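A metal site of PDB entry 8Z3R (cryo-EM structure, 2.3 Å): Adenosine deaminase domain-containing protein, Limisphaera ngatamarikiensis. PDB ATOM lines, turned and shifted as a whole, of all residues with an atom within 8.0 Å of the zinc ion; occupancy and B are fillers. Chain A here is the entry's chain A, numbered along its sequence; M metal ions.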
ATOM      1  N   HIS A 264     -11.663  16.647 -15.503  1.00  0.00           N
ATOM      2  CA  HIS A 264     -11.559  17.800 -14.607  1.00  0.00           C
ATOM      3  C   HIS A 264     -10.460  18.728 -15.115  1.00  0.00           C
ATOM      4  O   HIS A 264      -9.292  18.601 -14.712  1.00  0.00           O
ATOM      5  CB  HIS A 264     -11.303  17.365 -13.170  1.00  0.00           C
ATOM      6  CG  HIS A 264     -11.608  18.404 -12.153  1.00  0.00           C
ATOM      7  ND1 HIS A 264     -12.534  18.220 -11.146  1.00  0.00           N
ATOM      8  CD2 HIS A 264     -11.107  19.646 -11.964  1.00  0.00           C
ATOM      9  CE1 HIS A 264     -12.593  19.301 -10.393  1.00  0.00           C
ATOM     10  NE2 HIS A 264     -11.731  20.182 -10.867  1.00  0.00           N
ATOM     11  N   CYS A 265     -10.820  19.654 -15.999  1.00  0.00           N
ATOM     12  CA  CYS A 265      -9.865  20.595 -16.579  1.00  0.00           C
ATOM     13  C   CYS A 265     -10.513  21.969 -16.666  1.00  0.00           C
ATOM     14  O   CYS A 265     -11.624  22.098 -17.193  1.00  0.00           O
ATOM     15  CB  CYS A 265      -9.414  20.126 -17.965  1.00  0.00           C
ATOM     16  SG  CYS A 265      -7.916  20.932 -18.583  1.00  0.00           S
ATOM     17  N   HIS A 266      -9.832  22.986 -16.162  1.00  0.00           N
ATOM     18  CA  HIS A 266     -10.321  24.361 -16.184  1.00  0.00           C
ATOM     19  C   HIS A 266      -9.693  25.097 -17.365  1.00  0.00           C
ATOM     20  O   HIS A 266      -8.476  25.073 -17.543  1.00  0.00           O
ATOM     21  CB  HIS A 266      -9.987  25.080 -14.879  1.00  0.00           C
ATOM     22  CG  HIS A 266     -10.742  24.570 -13.689  1.00  0.00           C
ATOM     23  ND1 HIS A 266     -11.802  25.237 -13.132  1.00  0.00           N
ATOM     24  CD2 HIS A 266     -10.575  23.447 -12.954  1.00  0.00           C
ATOM     25  CE1 HIS A 266     -12.265  24.553 -12.106  1.00  0.00           C
ATOM     26  NE2 HIS A 266     -11.536  23.459 -11.968  1.00  0.00           N
ATOM     27  N   MET A 315      -4.817  30.480  -6.123  1.00  0.00           N
ATOM     28  CA  MET A 315      -5.627  31.169  -7.121  1.00  0.00           C
ATOM     29  C   MET A 315      -4.908  32.410  -7.658  1.00  0.00           C
ATOM     30  O   MET A 315      -4.994  32.711  -8.859  1.00  0.00           O
ATOM     31  CB  MET A 315      -6.983  31.552  -6.532  1.00  0.00           C
ATOM     32  CG  MET A 315      -7.857  30.355  -6.165  1.00  0.00           C
ATOM     33  SD  MET A 315      -8.326  29.365  -7.603  1.00  0.00           S
ATOM     34  CE  MET A 315      -9.101  27.966  -6.810  1.00  0.00           C
ATOM     35  N   ARG A 354     -14.201  22.961 -18.471  1.00  0.00           N
ATOM     36  CA  ARG A 354     -15.029  23.822 -17.640  1.00  0.00           C
ATOM     37  C   ARG A 354     -14.670  25.288 -17.867  1.00  0.00           C
ATOM     38  O   ARG A 354     -13.492  25.638 -17.916  1.00  0.00           O
ATOM     39  CB  ARG A 354     -14.863  23.458 -16.163  1.00  0.00           C
ATOM     40  CG  ARG A 354     -15.241  22.034 -15.834  1.00  0.00           C
ATOM     41  CD  ARG A 354     -14.984  21.705 -14.383  1.00  0.00           C
ATOM     42  NE  ARG A 354     -15.109  20.273 -14.132  1.00  0.00           N
ATOM     43  CZ  ARG A 354     -15.183  19.729 -12.928  1.00  0.00           C
ATOM     44  NH1 ARG A 354     -15.158  20.469 -11.830  1.00  0.00           N
ATOM     45  NH2 ARG A 354     -15.290  18.416 -12.817  1.00  0.00           N
ATOM     46  N   ILE A 401     -19.570  26.534 -15.012  1.00  0.00           N
ATOM     47  CA  ILE A 401     -19.194  26.635 -13.603  1.00  0.00           C
ATOM     48  C   ILE A 401     -20.067  27.672 -12.919  1.00  0.00           C
ATOM     49  O   ILE A 401     -20.273  28.778 -13.440  1.00  0.00           O
ATOM     50  CB  ILE A 401     -17.709  27.009 -13.453  1.00  0.00           C
ATOM     51  CG1 ILE A 401     -16.801  25.907 -13.997  1.00  0.00           C
ATOM     52  CG2 ILE A 401     -17.372  27.299 -11.999  1.00  0.00           C
ATOM     53  CD1 ILE A 401     -15.363  26.349 -14.154  1.00  0.00           C
ATOM     54  N   ASP A 440     -21.359  22.739 -12.908  1.00  0.00           N
ATOM     55  CA  ASP A 440     -20.433  22.534 -11.804  1.00  0.00           C
ATOM     56  C   ASP A 440     -20.698  23.570 -10.725  1.00  0.00           C
ATOM     57  O   ASP A 440     -21.042  24.723 -11.028  1.00  0.00           O
ATOM     58  CB  ASP A 440     -18.979  22.625 -12.274  1.00  0.00           C
ATOM     59  CG  ASP A 440     -18.005  22.103 -11.237  1.00  0.00           C
ATOM     60  OD1 ASP A 440     -16.785  22.164 -11.498  1.00  0.00           O
ATOM     61  OD2 ASP A 440     -18.449  21.634 -10.169  1.00  0.00           O
ATOM     62  N   LEU A 441     -20.530  23.170  -9.471  1.00  0.00           N
ATOM     63  CA  LEU A 441     -20.664  24.054  -8.315  1.00  0.00           C
ATOM     64  C   LEU A 441     -19.306  24.100  -7.622  1.00  0.00           C
ATOM     65  O   LEU A 441     -18.975  23.211  -6.820  1.00  0.00           O
ATOM     66  CB  LEU A 441     -21.764  23.579  -7.375  1.00  0.00           C
ATOM     67  CG  LEU A 441     -21.921  24.342  -6.066  1.00  0.00           C
ATOM     68  CD1 LEU A 441     -22.598  25.679  -6.297  1.00  0.00           C
ATOM     69  CD2 LEU A 441     -22.696  23.517  -5.049  1.00  0.00           C
ATOM     70  N   ALA A 442     -18.517  25.122  -7.926  1.00  0.00           N
ATOM     71  CA  ALA A 442     -17.172  25.276  -7.410  1.00  0.00           C
ATOM     72  C   ALA A 442     -17.047  26.588  -6.645  1.00  0.00           C
ATOM     73  O   ALA A 442     -18.030  27.308  -6.442  1.00  0.00           O
ATOM     74  CB  ALA A 442     -16.144  25.212  -8.543  1.00  0.00           C
ATOM     75  N   GLY A 443     -15.839  26.889  -6.218  1.00  0.00           N
ATOM     76  CA  GLY A 443     -15.541  28.110  -5.494  1.00  0.00           C
ATOM     77  C   GLY A 443     -15.207  27.848  -4.044  1.00  0.00           C
ATOM     78  O   GLY A 443     -14.961  26.723  -3.611  1.00  0.00           O
ATOM     79  N   HIS A 471     -17.875  20.396  -6.264  1.00  0.00           N
ATOM     80  CA  HIS A 471     -16.606  20.467  -5.524  1.00  0.00           C
ATOM     81  C   HIS A 471     -16.908  20.271  -4.048  1.00  0.00           C
ATOM     82  O   HIS A 471     -17.613  21.096  -3.446  1.00  0.00           O
ATOM     83  CB  HIS A 471     -15.918  21.796  -5.768  1.00  0.00           C
ATOM     84  CG  HIS A 471     -14.935  21.786  -6.900  1.00  0.00           C
ATOM     85  ND1 HIS A 471     -15.325  21.863  -8.224  1.00  0.00           N
ATOM     86  CD2 HIS A 471     -13.589  21.722  -6.918  1.00  0.00           C
ATOM     87  CE1 HIS A 471     -14.258  21.845  -9.005  1.00  0.00           C
ATOM     88  NE2 HIS A 471     -13.190  21.757  -8.231  1.00  0.00           N
ATOM     89  N   GLU A 474     -12.559  19.044  -0.329  1.00  0.00           N
ATOM     90  CA  GLU A 474     -11.181  19.539  -0.415  1.00  0.00           C
ATOM     91  C   GLU A 474     -10.783  20.266   0.864  1.00  0.00           C
ATOM     92  O   GLU A 474      -9.659  20.118   1.345  1.00  0.00           O
ATOM     93  CB  GLU A 474     -11.022  20.450  -1.626  1.00  0.00           C
ATOM     94  CG  GLU A 474      -9.608  20.956  -1.835  1.00  0.00           C
ATOM     95  CD  GLU A 474      -9.475  21.819  -3.082  1.00  0.00           C
ATOM     96  OE1 GLU A 474     -10.492  22.042  -3.761  1.00  0.00           O
ATOM     97  OE2 GLU A 474      -8.345  22.270  -3.363  1.00  0.00           O
ATOM     98  N   GLY A 494     -15.679  16.107  -6.778  1.00  0.00           N
ATOM     99  CA  GLY A 494     -14.324  16.556  -6.998  1.00  0.00           C
ATOM    100  C   GLY A 494     -13.602  16.775  -5.682  1.00  0.00           C
ATOM    101  O   GLY A 494     -14.139  17.413  -4.771  1.00  0.00           O
ATOM    102  N   HIS A 495     -12.382  16.245  -5.596  1.00  0.00           N
ATOM    103  CA  HIS A 495     -11.513  16.430  -4.429  1.00  0.00           C
ATOM    104  C   HIS A 495     -12.172  15.927  -3.144  1.00  0.00           C
ATOM    105  O   HIS A 495     -12.124  16.593  -2.113  1.00  0.00           O
ATOM    106  CB  HIS A 495     -11.089  17.898  -4.279  1.00  0.00           C
ATOM    107  CG  HIS A 495     -10.337  18.433  -5.450  1.00  0.00           C
ATOM    108  ND1 HIS A 495     -10.563  19.699  -5.963  1.00  0.00           N
ATOM    109  CD2 HIS A 495      -9.361  17.895  -6.218  1.00  0.00           C
ATOM    110  CE1 HIS A 495      -9.757  19.904  -6.991  1.00  0.00           C
ATOM    111  NE2 HIS A 495      -9.027  18.819  -7.169  1.00  0.00           N
ATOM    112  N   GLU A 517     -13.139  12.375  -8.546  1.00  0.00           N
ATOM    113  CA  GLU A 517     -12.054  12.937  -9.351  1.00  0.00           C
ATOM    114  C   GLU A 517     -10.947  13.422  -8.430  1.00  0.00           C
ATOM    115  O   GLU A 517     -11.208  14.221  -7.521  1.00  0.00           O
ATOM    116  CB  GLU A 517     -12.576  14.077 -10.227  1.00  0.00           C
ATOM    117  CG  GLU A 517     -13.892  13.772 -10.916  1.00  0.00           C
ATOM    118  CD  GLU A 517     -14.692  15.022 -11.230  1.00  0.00           C
ATOM    119  OE1 GLU A 517     -14.370  16.089 -10.667  1.00  0.00           O
ATOM    120  OE2 GLU A 517     -15.652  14.932 -12.027  1.00  0.00           O
ATOM    121  N   CYS A 519      -6.829  14.976  -8.128  1.00  0.00           N
ATOM    122  CA  CYS A 519      -5.784  15.741  -8.823  1.00  0.00           C
ATOM    123  C   CYS A 519      -4.501  15.663  -8.014  1.00  0.00           C
ATOM    124  O   CYS A 519      -4.271  16.503  -7.130  1.00  0.00           O
ATOM    125  CB  CYS A 519      -6.218  17.189  -9.018  1.00  0.00           C
ATOM    126  SG  CYS A 519      -7.942  17.402  -9.513  1.00  0.00           S
ATOM    127  N   THR A 568      -6.142  16.674 -13.991  1.00  0.00           N
ATOM    128  CA  THR A 568      -5.106  17.690 -13.916  1.00  0.00           C
ATOM    129  C   THR A 568      -5.493  18.937 -13.139  1.00  0.00           C
ATOM    130  O   THR A 568      -4.603  19.658 -12.687  1.00  0.00           O
ATOM    131  CB  THR A 568      -4.678  18.131 -15.331  1.00  0.00           C
ATOM    132  OG1 THR A 568      -5.808  18.700 -16.017  1.00  0.00           O
ATOM    133  CG2 THR A 568      -4.142  16.964 -16.124  1.00  0.00           C
ATOM    134  N   ASP A 569      -6.783  19.223 -13.000  1.00  0.00           N
ATOM    135  CA  ASP A 569      -7.266  20.488 -12.422  1.00  0.00           C
ATOM    136  C   ASP A 569      -6.780  21.625 -13.308  1.00  0.00           C
ATOM    137  O   ASP A 569      -7.175  21.681 -14.482  1.00  0.00           O
ATOM    138  CB  ASP A 569      -6.864  20.571 -10.945  1.00  0.00           C
ATOM    139  CG  ASP A 569      -7.902  21.260 -10.087  1.00  0.00           C
ATOM    140  OD1 ASP A 569      -9.079  21.310 -10.501  1.00  0.00           O
ATOM    141  OD2 ASP A 569      -7.532  21.759  -9.006  1.00  0.00           O
ATOM    142  N   ASN A 570      -5.939  22.536 -12.814  1.00  0.00           N
ATOM    143  CA  ASN A 570      -5.412  23.625 -13.630  1.00  0.00           C
ATOM    144  C   ASN A 570      -4.060  23.227 -14.186  1.00  0.00           C
ATOM    145  O   ASN A 570      -3.111  22.982 -13.422  1.00  0.00           O
ATOM    146  CB  ASN A 570      -5.303  24.903 -12.808  1.00  0.00           C
ATOM    147  CG  ASN A 570      -6.643  25.379 -12.279  1.00  0.00           C
ATOM    148  OD1 ASN A 570      -7.069  24.985 -11.196  1.00  0.00           O
ATOM    149  ND2 ASN A 570      -7.314  26.231 -13.056  1.00  0.00           N
HETATM  150 ZN    ZN M   1     -11.822  22.310 -10.002  1.00  0.00          ZN
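Merely in contact with the zinc ion: Asp 569 (3.0 Å).
Of the 19 residues printed, 4 come within 4 Å of the zinc ion.
The nearest printed residue that does not touch the zinc ion is Arg 354 (4.2 Å).
The zinc ion is bound by a ring nitrogen (NE2) of His 266 (2.3 Å), a ring nitrogen (NE2) of His 264 (2.3 Å) and a ring nitrogen (NE2) of His 471 (2.3 Å).
The zinc ion has three donor atoms within binding distance.
NH2 of Arg 354 is in hydrogen-bond range of ND1 of His 264 (3.2 Å).
N of His 471 is in hydrogen-bond range of O of Leu 441 (3.1 Å).
The backbone carbonyl oxygen of Asp 569 lies within hydrogen-bond range of the backbone NH of His 266 (3.4 Å).
ND1 of His 264 is in hydrogen-bond range of OE1 of Glu 517, 2.9 Å away.
The backbone NH (N) of Asp 569 sits at hydrogen-bond distance from the backbone carbonyl oxygen (O) of His 264, 3.1 Å away.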
